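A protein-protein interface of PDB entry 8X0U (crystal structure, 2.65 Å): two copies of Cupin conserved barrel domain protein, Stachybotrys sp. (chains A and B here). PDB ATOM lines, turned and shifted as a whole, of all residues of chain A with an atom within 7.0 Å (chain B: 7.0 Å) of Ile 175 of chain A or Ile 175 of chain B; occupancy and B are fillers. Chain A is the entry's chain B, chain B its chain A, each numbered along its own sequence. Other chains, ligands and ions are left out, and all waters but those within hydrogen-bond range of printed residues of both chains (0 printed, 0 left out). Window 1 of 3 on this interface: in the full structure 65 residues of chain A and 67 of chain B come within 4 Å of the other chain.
N of Leu 177 of chain A sits at hydrogen-bond distance from O of Ile 122 of chain A (3.0 Å).
N of Ile 126 of chain B is in hydrogen-bond range of O of Met 173 of chain B (3.1 Å).
O of Met 173 of chain A sits at hydrogen-bond distance from N of Ile 126 of chain A (2.9 Å).
The backbone carbonyl oxygen of Ile 122 of chain B sits at hydrogen-bond distance from the backbone NH of Leu 177 of chain B, at 3.1 Å.
The backbone carbonyl oxygen of Tyr 124 of chain A is in hydrogen-bond range of the backbone NH of Ile 175 of chain A, at 2.8 Å.
The backbone carbonyl oxygen (O) of Tyr 124 of chain B lies within hydrogen-bond range of the backbone NH (N) of Ile 175 of chain B, 2.8 Å away.
Ile 175 of chain A touches just one residue of chain B: Ile 175.
Ile 175 of chain B touches one residue of chain A.
Of the printed residues of chain B, Ile 126 of chain A touches Met 173 (3.5 Å).
Of the printed residues of chain A, Ser 101 of chain B touches Tyr 124 and Leu 177.
Ser 121 of chain A touches none of the printed residues of chain B.
Ile 102 of chain A touches none of the printed residues of chain B.
The nearest residue of chain B that does not touch Ile 175 of chain A is Tyr 124 of chain B (4.3 Å).
The nearest printed residue of chain B that does not touch Ser 101 of chain A is Ile 122 of chain B (6.7 Å).
The side-chain hydroxyl (OG) of Ser 101 of chain B sits at hydrogen-bond distance from the side-chain hydroxyl (OH) of Tyr 124 of chain A, at 2.8 Å.
The side-chain hydroxyl of Ser 101 of chain A is in hydrogen-bond range of the side-chain hydroxyl of Tyr 124 of chain B (2.7 Å).
Among the printed residues, pairs that only touch across the chains: Leu 177 of chain A with Ser 101 of chain B (3.4 Å), Ile 126 of chain A with Met 173 of chain B (3.5 Å), Val 103 of chain A with Tyr 124 of chain B (3.5 Å), Tyr 124 of chain A with Val 103 of chain B (3.5 Å), Ile 175 of chain A with Ile 175 of chain B (3.7 Å), Met 173 of chain A with Ile 126 of chain B (3.7 Å) and Ser 101 of chain A with Leu 177 of chain B (3.8 Å).
Printed residues of chain A that touch a printed residue of chain B: Ser 101, Val 103, Tyr 124, Ile 126, Met 173, Ile 175 and Leu 177.
Hydrophobic or aromatic side chains of chain A that line the printed part of chain B: Val 103, Tyr 124, Ile 126, Met 173, Ile 175 and Leu 177.
Hydrophobic or aromatic side chains of chain B that line the printed part of chain A: Val 103, Tyr 124, Ile 126, Met 173, Ile 175 and Leu 177.
Among the printed residues, no Asp or Glu carboxylate lies within 4 Å of a Lys or Arg side-chain nitrogen of the other chain.
Ser 101 of chain A touches Tyr 124 of chain B, and with the chains exchanged Tyr 124 of chain A touches Ser 101 of chain B.
Ser 101 of chain A touches Leu 177 of chain B, and with the chains exchanged Leu 177 of chain A touches Ser 101 of chain B.
Val 103 of chain A touches Tyr 124 of chain B, and with the chains exchanged Tyr 124 of chain A touches Val 103 of chain B.
Ile 175 of chain B touches its own counterpart, Ile 175 of chain A.
Of the 9 pairs that touch across the chains among the printed residues, 9 have their exchanged pair printed and touching as well.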
ATOM      1  N   SER A 101      25.586 -12.197 -14.543  1.00  0.00           N
ATOM      2  CA  SER A 101      26.559 -12.257 -15.623  1.00  0.00           C
ATOM      3  C   SER A 101      27.940 -12.521 -15.048  1.00  0.00           C
ATOM      4  O   SER A 101      28.210 -12.238 -13.880  1.00  0.00           O
ATOM      5  CB  SER A 101      26.575 -10.957 -16.437  1.00  0.00           C
ATOM      6  OG  SER A 101      27.047  -9.876 -15.652  1.00  0.00           O
ATOM      7  N   ILE A 102      28.807 -13.090 -15.883  1.00  0.00           N
ATOM      8  CA  ILE A 102      30.220 -13.269 -15.566  1.00  0.00           C
ATOM      9  C   ILE A 102      31.024 -12.965 -16.819  1.00  0.00           C
ATOM     10  O   ILE A 102      30.736 -13.503 -17.894  1.00  0.00           O
ATOM     11  CB  ILE A 102      30.541 -14.693 -15.072  1.00  0.00           C
ATOM     12  CG1 ILE A 102      29.672 -15.073 -13.875  1.00  0.00           C
ATOM     13  CG2 ILE A 102      32.019 -14.808 -14.718  1.00  0.00           C
ATOM     14  CD1 ILE A 102      30.118 -16.331 -13.179  1.00  0.00           C
ATOM     15  N   VAL A 103      32.025 -12.102 -16.690  1.00  0.00           N
ATOM     16  CA  VAL A 103      32.999 -11.867 -17.748  1.00  0.00           C
ATOM     17  C   VAL A 103      34.238 -12.677 -17.400  1.00  0.00           C
ATOM     18  O   VAL A 103      34.994 -12.313 -16.490  1.00  0.00           O
ATOM     19  CB  VAL A 103      33.331 -10.377 -17.902  1.00  0.00           C
ATOM     20  CG1 VAL A 103      34.089 -10.141 -19.200  1.00  0.00           C
ATOM     21  CG2 VAL A 103      32.063  -9.549 -17.865  1.00  0.00           C
ATOM     22  N   ARG A 104      34.450 -13.779 -18.111  1.00  0.00           N
ATOM     23  CA  ARG A 104      35.558 -14.685 -17.842  1.00  0.00           C
ATOM     24  C   ARG A 104      36.551 -14.624 -18.994  1.00  0.00           C
ATOM     25  O   ARG A 104      36.193 -14.904 -20.143  1.00  0.00           O
ATOM     26  CB  ARG A 104      35.059 -16.114 -17.634  1.00  0.00           C
ATOM     27  CG  ARG A 104      36.153 -17.080 -17.206  1.00  0.00           C
ATOM     28  CD  ARG A 104      35.584 -18.368 -16.639  1.00  0.00           C
ATOM     29  NE  ARG A 104      34.990 -18.173 -15.322  1.00  0.00           N
ATOM     30  CZ  ARG A 104      33.695 -18.317 -15.060  1.00  0.00           C
ATOM     31  NH1 ARG A 104      32.856 -18.657 -16.028  1.00  0.00           N
ATOM     32  NH2 ARG A 104      33.239 -18.121 -13.831  1.00  0.00           N
ATOM     33  N   SER A 121      23.968 -22.093 -19.882  1.00  0.00           N
ATOM     34  CA  SER A 121      24.060 -20.646 -19.975  1.00  0.00           C
ATOM     35  C   SER A 121      24.268 -20.304 -21.441  1.00  0.00           C
ATOM     36  O   SER A 121      24.634 -21.164 -22.245  1.00  0.00           O
ATOM     37  CB  SER A 121      25.205 -20.092 -19.116  1.00  0.00           C
ATOM     38  OG  SER A 121      26.464 -20.546 -19.584  1.00  0.00           O
ATOM     39  N   ILE A 122      24.027 -19.046 -21.786  1.00  0.00           N
ATOM     40  CA  ILE A 122      24.355 -18.542 -23.112  1.00  0.00           C
ATOM     41  C   ILE A 122      25.630 -17.715 -22.987  1.00  0.00           C
ATOM     42  O   ILE A 122      25.704 -16.783 -22.177  1.00  0.00           O
ATOM     43  CB  ILE A 122      23.195 -17.739 -23.723  1.00  0.00           C
ATOM     44  CG1 ILE A 122      23.586 -17.205 -25.103  1.00  0.00           C
ATOM     45  CG2 ILE A 122      22.727 -16.623 -22.793  1.00  0.00           C
ATOM     46  CD1 ILE A 122      22.399 -16.840 -25.969  1.00  0.00           C
ATOM     47  N   ASP A 123      26.648 -18.075 -23.765  1.00  0.00           N
ATOM     48  CA  ASP A 123      27.988 -17.520 -23.620  1.00  0.00           C
ATOM     49  C   ASP A 123      28.345 -16.713 -24.859  1.00  0.00           C
ATOM     50  O   ASP A 123      28.345 -17.251 -25.973  1.00  0.00           O
ATOM     51  CB  ASP A 123      29.021 -18.628 -23.393  1.00  0.00           C
ATOM     52  CG  ASP A 123      28.572 -19.643 -22.359  1.00  0.00           C
ATOM     53  OD1 ASP A 123      27.803 -19.264 -21.449  1.00  0.00           O
ATOM     54  OD2 ASP A 123      28.993 -20.820 -22.460  1.00  0.00           O
ATOM     55  N   TYR A 124      28.653 -15.432 -24.664  1.00  0.00           N
ATOM     56  CA  TYR A 124      29.190 -14.579 -25.720  1.00  0.00           C
ATOM     57  C   TYR A 124      30.711 -14.645 -25.657  1.00  0.00           C
ATOM     58  O   TYR A 124      31.326 -14.039 -24.773  1.00  0.00           O
ATOM     59  CB  TYR A 124      28.722 -13.135 -25.563  1.00  0.00           C
ATOM     60  CG  TYR A 124      27.227 -12.910 -25.552  1.00  0.00           C
ATOM     61  CD1 TYR A 124      26.391 -13.558 -26.453  1.00  0.00           C
ATOM     62  CD2 TYR A 124      26.655 -12.022 -24.649  1.00  0.00           C
ATOM     63  CE1 TYR A 124      25.024 -13.336 -26.442  1.00  0.00           C
ATOM     64  CE2 TYR A 124      25.293 -11.793 -24.631  1.00  0.00           C
ATOM     65  CZ  TYR A 124      24.480 -12.452 -25.529  1.00  0.00           C
ATOM     66  OH  TYR A 124      23.123 -12.227 -25.513  1.00  0.00           O
ATOM     67  N   GLY A 125      31.322 -15.357 -26.594  1.00  0.00           N
ATOM     68  CA  GLY A 125      32.767 -15.534 -26.628  1.00  0.00           C
ATOM     69  C   GLY A 125      33.392 -14.805 -27.806  1.00  0.00           C
ATOM     70  O   GLY A 125      32.823 -14.774 -28.900  1.00  0.00           O
ATOM     71  N   ILE A 126      34.563 -14.214 -27.565  1.00  0.00           N
ATOM     72  CA  ILE A 126      35.361 -13.576 -28.604  1.00  0.00           C
ATOM     73  C   ILE A 126      36.809 -14.020 -28.436  1.00  0.00           C
ATOM     74  O   ILE A 126      37.284 -14.251 -27.320  1.00  0.00           O
ATOM     75  CB  ILE A 126      35.247 -12.033 -28.559  1.00  0.00           C
ATOM     76  CG1 ILE A 126      36.262 -11.385 -29.508  1.00  0.00           C
ATOM     77  CG2 ILE A 126      35.434 -11.525 -27.142  1.00  0.00           C
ATOM     78  CD1 ILE A 126      35.853 -10.043 -30.044  1.00  0.00           C
ATOM     79  N   MET A 173      37.672 -14.561 -24.308  1.00  0.00           N
ATOM     80  CA  MET A 173      36.867 -13.855 -23.320  1.00  0.00           C
ATOM     81  C   MET A 173      35.404 -14.195 -23.544  1.00  0.00           C
ATOM     82  O   MET A 173      34.900 -14.085 -24.666  1.00  0.00           O
ATOM     83  CB  MET A 173      37.070 -12.336 -23.393  1.00  0.00           C
ATOM     84  CG  MET A 173      36.263 -11.577 -22.352  1.00  0.00           C
ATOM     85  SD  MET A 173      36.572  -9.801 -22.349  1.00  0.00           S
ATOM     86  CE  MET A 173      35.359  -9.251 -23.547  1.00  0.00           C
ATOM     87  N   TRP A 174      34.730 -14.613 -22.478  1.00  0.00           N
ATOM     88  CA  TRP A 174      33.318 -14.948 -22.528  1.00  0.00           C
ATOM     89  C   TRP A 174      32.518 -14.004 -21.642  1.00  0.00           C
ATOM     90  O   TRP A 174      33.041 -13.400 -20.701  1.00  0.00           O
ATOM     91  CB  TRP A 174      33.065 -16.391 -22.078  1.00  0.00           C
ATOM     92  CG  TRP A 174      33.633 -17.429 -22.983  1.00  0.00           C
ATOM     93  CD1 TRP A 174      33.036 -17.979 -24.080  1.00  0.00           C
ATOM     94  CD2 TRP A 174      34.911 -18.060 -22.862  1.00  0.00           C
ATOM     95  NE1 TRP A 174      33.868 -18.910 -24.654  1.00  0.00           N
ATOM     96  CE2 TRP A 174      35.025 -18.979 -23.924  1.00  0.00           C
ATOM     97  CE3 TRP A 174      35.971 -17.935 -21.961  1.00  0.00           C
ATOM     98  CZ2 TRP A 174      36.157 -19.768 -24.108  1.00  0.00           C
ATOM     99  CZ3 TRP A 174      37.093 -18.717 -22.147  1.00  0.00           C
ATOM    100  CH2 TRP A 174      37.177 -19.625 -23.209  1.00  0.00           C
ATOM    101  N   ILE A 175      31.236 -13.880 -21.968  1.00  0.00           N
ATOM    102  CA  ILE A 175      30.245 -13.294 -21.077  1.00  0.00           C
ATOM    103  C   ILE A 175      29.133 -14.318 -20.921  1.00  0.00           C
ATOM    104  O   ILE A 175      28.449 -14.650 -21.897  1.00  0.00           O
ATOM    105  CB  ILE A 175      29.700 -11.957 -21.598  1.00  0.00           C
ATOM    106  CG1 ILE A 175      30.795 -10.889 -21.590  1.00  0.00           C
ATOM    107  CG2 ILE A 175      28.520 -11.505 -20.749  1.00  0.00           C
ATOM    108  CD1 ILE A 175      31.498 -10.720 -22.915  1.00  0.00           C
ATOM    109  N   LEU A 176      28.966 -14.831 -19.709  1.00  0.00           N
ATOM    110  CA  LEU A 176      28.012 -15.894 -19.433  1.00  0.00           C
ATOM    111  C   LEU A 176      26.742 -15.302 -18.840  1.00  0.00           C
ATOM    112  O   LEU A 176      26.799 -14.559 -17.857  1.00  0.00           O
ATOM    113  CB  LEU A 176      28.612 -16.929 -18.479  1.00  0.00           C
ATOM    114  CG  LEU A 176      29.713 -17.834 -19.043  1.00  0.00           C
ATOM    115  CD1 LEU A 176      31.084 -17.190 -18.893  1.00  0.00           C
ATOM    116  CD2 LEU A 176      29.685 -19.196 -18.365  1.00  0.00           C
ATOM    117  N   LEU A 177      25.604 -15.627 -19.447  1.00  0.00           N
ATOM    118  CA  LEU A 177      24.302 -15.190 -18.971  1.00  0.00           C
ATOM    119  C   LEU A 177      23.450 -16.405 -18.635  1.00  0.00           C
ATOM    120  O   LEU A 177      23.585 -17.465 -19.252  1.00  0.00           O
ATOM    121  CB  LEU A 177      23.573 -14.332 -20.016  1.00  0.00           C
ATOM    122  CG  LEU A 177      24.263 -13.071 -20.537  1.00  0.00           C
ATOM    123  CD1 LEU A 177      23.344 -12.337 -21.498  1.00  0.00           C
ATOM    124  CD2 LEU A 177      24.677 -12.163 -19.390  1.00  0.00           C
ATOM    125  N   SER B 101      20.149  -8.287 -22.910  1.00  0.00           N
ATOM    126  CA  SER B 101      21.506  -7.976 -23.331  1.00  0.00           C
ATOM    127  C   SER B 101      21.522  -7.580 -24.801  1.00  0.00           C
ATOM    128  O   SER B 101      20.632  -7.939 -25.575  1.00  0.00           O
ATOM    129  CB  SER B 101      22.445  -9.169 -23.111  1.00  0.00           C
ATOM    130  OG  SER B 101      22.024 -10.292 -23.865  1.00  0.00           O
ATOM    131  N   ILE B 102      22.554  -6.820 -25.170  1.00  0.00           N
ATOM    132  CA  ILE B 102      22.841  -6.468 -26.557  1.00  0.00           C
ATOM    133  C   ILE B 102      24.352  -6.472 -26.737  1.00  0.00           C
ATOM    134  O   ILE B 102      25.073  -5.818 -25.975  1.00  0.00           O
ATOM    135  CB  ILE B 102      22.269  -5.092 -26.957  1.00  0.00           C
ATOM    136  CG1 ILE B 102      20.760  -5.023 -26.717  1.00  0.00           C
ATOM    137  CG2 ILE B 102      22.577  -4.794 -28.420  1.00  0.00           C
ATOM    138  CD1 ILE B 102      20.138  -3.735 -27.188  1.00  0.00           C
ATOM    139  N   VAL B 103      24.833  -7.200 -27.735  1.00  0.00           N
ATOM    140  CA  VAL B 103      26.246  -7.206 -28.092  1.00  0.00           C
ATOM    141  C   VAL B 103      26.385  -6.355 -29.347  1.00  0.00           C
ATOM    142  O   VAL B 103      26.103  -6.814 -30.458  1.00  0.00           O
ATOM    143  CB  VAL B 103      26.781  -8.625 -28.304  1.00  0.00           C
ATOM    144  CG1 VAL B 103      28.274  -8.589 -28.598  1.00  0.00           C
ATOM    145  CG2 VAL B 103      26.500  -9.487 -27.091  1.00  0.00           C
ATOM    146  N   ARG B 104      26.825  -5.110 -29.173  1.00  0.00           N
ATOM    147  CA  ARG B 104      26.946  -4.156 -30.267  1.00  0.00           C
ATOM    148  C   ARG B 104      28.419  -3.916 -30.570  1.00  0.00           C
ATOM    149  O   ARG B 104      29.188  -3.537 -29.681  1.00  0.00           O
ATOM    150  CB  ARG B 104      26.242  -2.842 -29.929  1.00  0.00           C
ATOM    151  CG  ARG B 104      26.298  -1.804 -31.042  1.00  0.00           C
ATOM    152  CD  ARG B 104      25.474  -0.573 -30.696  1.00  0.00           C
ATOM    153  NE  ARG B 104      24.045  -0.872 -30.643  1.00  0.00           N
ATOM    154  CZ  ARG B 104      23.318  -0.862 -29.531  1.00  0.00           C
ATOM    155  NH1 ARG B 104      23.880  -0.565 -28.367  1.00  0.00           N
ATOM    156  NH2 ARG B 104      22.023  -1.145 -29.582  1.00  0.00           N
ATOM    157  N   SER B 121      22.757   1.876 -18.296  1.00  0.00           N
ATOM    158  CA  SER B 121      23.044   0.472 -18.541  1.00  0.00           C
ATOM    159  C   SER B 121      24.499   0.240 -18.171  1.00  0.00           C
ATOM    160  O   SER B 121      25.341   1.126 -18.354  1.00  0.00           O
ATOM    161  CB  SER B 121      22.799   0.088 -20.006  1.00  0.00           C
ATOM    162  OG  SER B 121      23.624   0.844 -20.881  1.00  0.00           O
ATOM    163  N   ILE B 122      24.788  -0.945 -17.648  1.00  0.00           N
ATOM    164  CA  ILE B 122      26.162  -1.341 -17.368  1.00  0.00           C
ATOM    165  C   ILE B 122      26.729  -1.985 -18.628  1.00  0.00           C
ATOM    166  O   ILE B 122      26.165  -2.951 -19.154  1.00  0.00           O
ATOM    167  CB  ILE B 122      26.246  -2.288 -16.161  1.00  0.00           C
ATOM    168  CG1 ILE B 122      27.672  -2.824 -16.001  1.00  0.00           C
ATOM    169  CG2 ILE B 122      25.234  -3.427 -16.271  1.00  0.00           C
ATOM    170  CD1 ILE B 122      28.085  -3.050 -14.558  1.00  0.00           C
ATOM    171  N   ASP B 123      27.834  -1.436 -19.125  1.00  0.00           N
ATOM    172  CA  ASP B 123      28.386  -1.815 -20.420  1.00  0.00           C
ATOM    173  C   ASP B 123      29.779  -2.396 -20.230  1.00  0.00           C
ATOM    174  O   ASP B 123      30.685  -1.699 -19.760  1.00  0.00           O
ATOM    175  CB  ASP B 123      28.440  -0.612 -21.367  1.00  0.00           C
ATOM    176  CG  ASP B 123      27.122   0.142 -21.442  1.00  0.00           C
ATOM    177  OD1 ASP B 123      26.058  -0.489 -21.259  1.00  0.00           O
ATOM    178  OD2 ASP B 123      27.151   1.367 -21.692  1.00  0.00           O
ATOM    179  N   TYR B 124      29.942  -3.669 -20.587  1.00  0.00           N
ATOM    180  CA  TYR B 124      31.268  -4.247 -20.751  1.00  0.00           C
ATOM    181  C   TYR B 124      31.782  -3.910 -22.143  1.00  0.00           C
ATOM    182  O   TYR B 124      31.099  -4.164 -23.141  1.00  0.00           O
ATOM    183  CB  TYR B 124      31.239  -5.765 -20.568  1.00  0.00           C
ATOM    184  CG  TYR B 124      30.549  -6.264 -19.322  1.00  0.00           C
ATOM    185  CD1 TYR B 124      30.777  -5.673 -18.084  1.00  0.00           C
ATOM    186  CD2 TYR B 124      29.684  -7.348 -19.382  1.00  0.00           C
ATOM    187  CE1 TYR B 124      30.146  -6.144 -16.943  1.00  0.00           C
ATOM    188  CE2 TYR B 124      29.053  -7.824 -18.253  1.00  0.00           C
ATOM    189  CZ  TYR B 124      29.285  -7.222 -17.036  1.00  0.00           C
ATOM    190  OH  TYR B 124      28.651  -7.707 -15.916  1.00  0.00           O
ATOM    191  N   GLY B 125      32.970  -3.343 -22.214  1.00  0.00           N
ATOM    192  CA  GLY B 125      33.565  -2.979 -23.490  1.00  0.00           C
ATOM    193  C   GLY B 125      34.987  -3.479 -23.604  1.00  0.00           C
ATOM    194  O   GLY B 125      35.760  -3.410 -22.651  1.00  0.00           O
ATOM    195  N   ILE B 126      35.323  -3.988 -24.787  1.00  0.00           N
ATOM    196  CA  ILE B 126      36.675  -4.438 -25.096  1.00  0.00           C
ATOM    197  C   ILE B 126      37.083  -3.843 -26.436  1.00  0.00           C
ATOM    198  O   ILE B 126      36.294  -3.844 -27.388  1.00  0.00           O
ATOM    199  CB  ILE B 126      36.783  -5.976 -25.117  1.00  0.00           C
ATOM    200  CG1 ILE B 126      38.217  -6.406 -25.442  1.00  0.00           C
ATOM    201  CG2 ILE B 126      35.787  -6.592 -26.100  1.00  0.00           C
ATOM    202  CD1 ILE B 126      38.511  -7.854 -25.126  1.00  0.00           C
ATOM    203  N   MET B 173      33.759  -3.435 -29.168  1.00  0.00           N
ATOM    204  CA  MET B 173      32.594  -4.264 -28.902  1.00  0.00           C
ATOM    205  C   MET B 173      32.077  -3.972 -27.504  1.00  0.00           C
ATOM    206  O   MET B 173      32.859  -3.752 -26.576  1.00  0.00           O
ATOM    207  CB  MET B 173      32.890  -5.757 -29.026  1.00  0.00           C
ATOM    208  CG  MET B 173      31.645  -6.605 -28.799  1.00  0.00           C
ATOM    209  SD  MET B 173      31.992  -8.339 -28.527  1.00  0.00           S
ATOM    210  CE  MET B 173      32.647  -8.722 -30.132  1.00  0.00           C
ATOM    211  N   TRP B 174      30.756  -3.979 -27.363  1.00  0.00           N
ATOM    212  CA  TRP B 174      30.102  -3.738 -26.089  1.00  0.00           C
ATOM    213  C   TRP B 174      29.068  -4.821 -25.827  1.00  0.00           C
ATOM    214  O   TRP B 174      28.501  -5.400 -26.757  1.00  0.00           O
ATOM    215  CB  TRP B 174      29.418  -2.373 -26.061  1.00  0.00           C
ATOM    216  CG  TRP B 174      30.362  -1.231 -25.967  1.00  0.00           C
ATOM    217  CD1 TRP B 174      31.045  -0.821 -24.860  1.00  0.00           C
ATOM    218  CD2 TRP B 174      30.730  -0.335 -27.020  1.00  0.00           C
ATOM    219  NE1 TRP B 174      31.817   0.274 -25.159  1.00  0.00           N
ATOM    220  CE2 TRP B 174      31.641   0.591 -26.480  1.00  0.00           C
ATOM    221  CE3 TRP B 174      30.378  -0.228 -28.368  1.00  0.00           C
ATOM    222  CZ2 TRP B 174      32.205   1.614 -27.240  1.00  0.00           C
ATOM    223  CZ3 TRP B 174      30.939   0.786 -29.120  1.00  0.00           C
ATOM    224  CH2 TRP B 174      31.839   1.695 -28.554  1.00  0.00           C
ATOM    225  N   ILE B 175      28.841  -5.091 -24.547  1.00  0.00           N
ATOM    226  CA  ILE B 175      27.714  -5.892 -24.089  1.00  0.00           C
ATOM    227  C   ILE B 175      26.938  -5.020 -23.112  1.00  0.00           C
ATOM    228  O   ILE B 175      27.440  -4.688 -22.031  1.00  0.00           O
ATOM    229  CB  ILE B 175      28.153  -7.211 -23.436  1.00  0.00           C
ATOM    230  CG1 ILE B 175      28.614  -8.214 -24.497  1.00  0.00           C
ATOM    231  CG2 ILE B 175      27.011  -7.812 -22.636  1.00  0.00           C
ATOM    232  CD1 ILE B 175      30.051  -8.039 -24.938  1.00  0.00           C
ATOM    233  N   LEU B 176      25.724  -4.634 -23.497  1.00  0.00           N
ATOM    234  CA  LEU B 176      24.911  -3.699 -22.729  1.00  0.00           C
ATOM    235  C   LEU B 176      23.850  -4.477 -21.961  1.00  0.00           C
ATOM    236  O   LEU B 176      22.960  -5.087 -22.561  1.00  0.00           O
ATOM    237  CB  LEU B 176      24.272  -2.656 -23.642  1.00  0.00           C
ATOM    238  CG  LEU B 176      25.213  -1.663 -24.332  1.00  0.00           C
ATOM    239  CD1 LEU B 176      25.540  -2.117 -25.745  1.00  0.00           C
ATOM    240  CD2 LEU B 176      24.613  -0.261 -24.338  1.00  0.00           C
ATOM    241  N   LEU B 177      23.945  -4.448 -20.636  1.00  0.00           N
ATOM    242  CA  LEU B 177      22.982  -5.099 -19.764  1.00  0.00           C
ATOM    243  C   LEU B 177      22.157  -4.054 -19.023  1.00  0.00           C
ATOM    244  O   LEU B 177      22.567  -2.900 -18.869  1.00  0.00           O
ATOM    245  CB  LEU B 177      23.682  -6.023 -18.763  1.00  0.00           C
ATOM    246  CG  LEU B 177      24.696  -7.005 -19.355  1.00  0.00           C
ATOM    247  CD1 LEU B 177      25.569  -7.602 -18.267  1.00  0.00           C
ATOM    248  CD2 LEU B 177      23.980  -8.096 -20.117  1.00  0.00           C
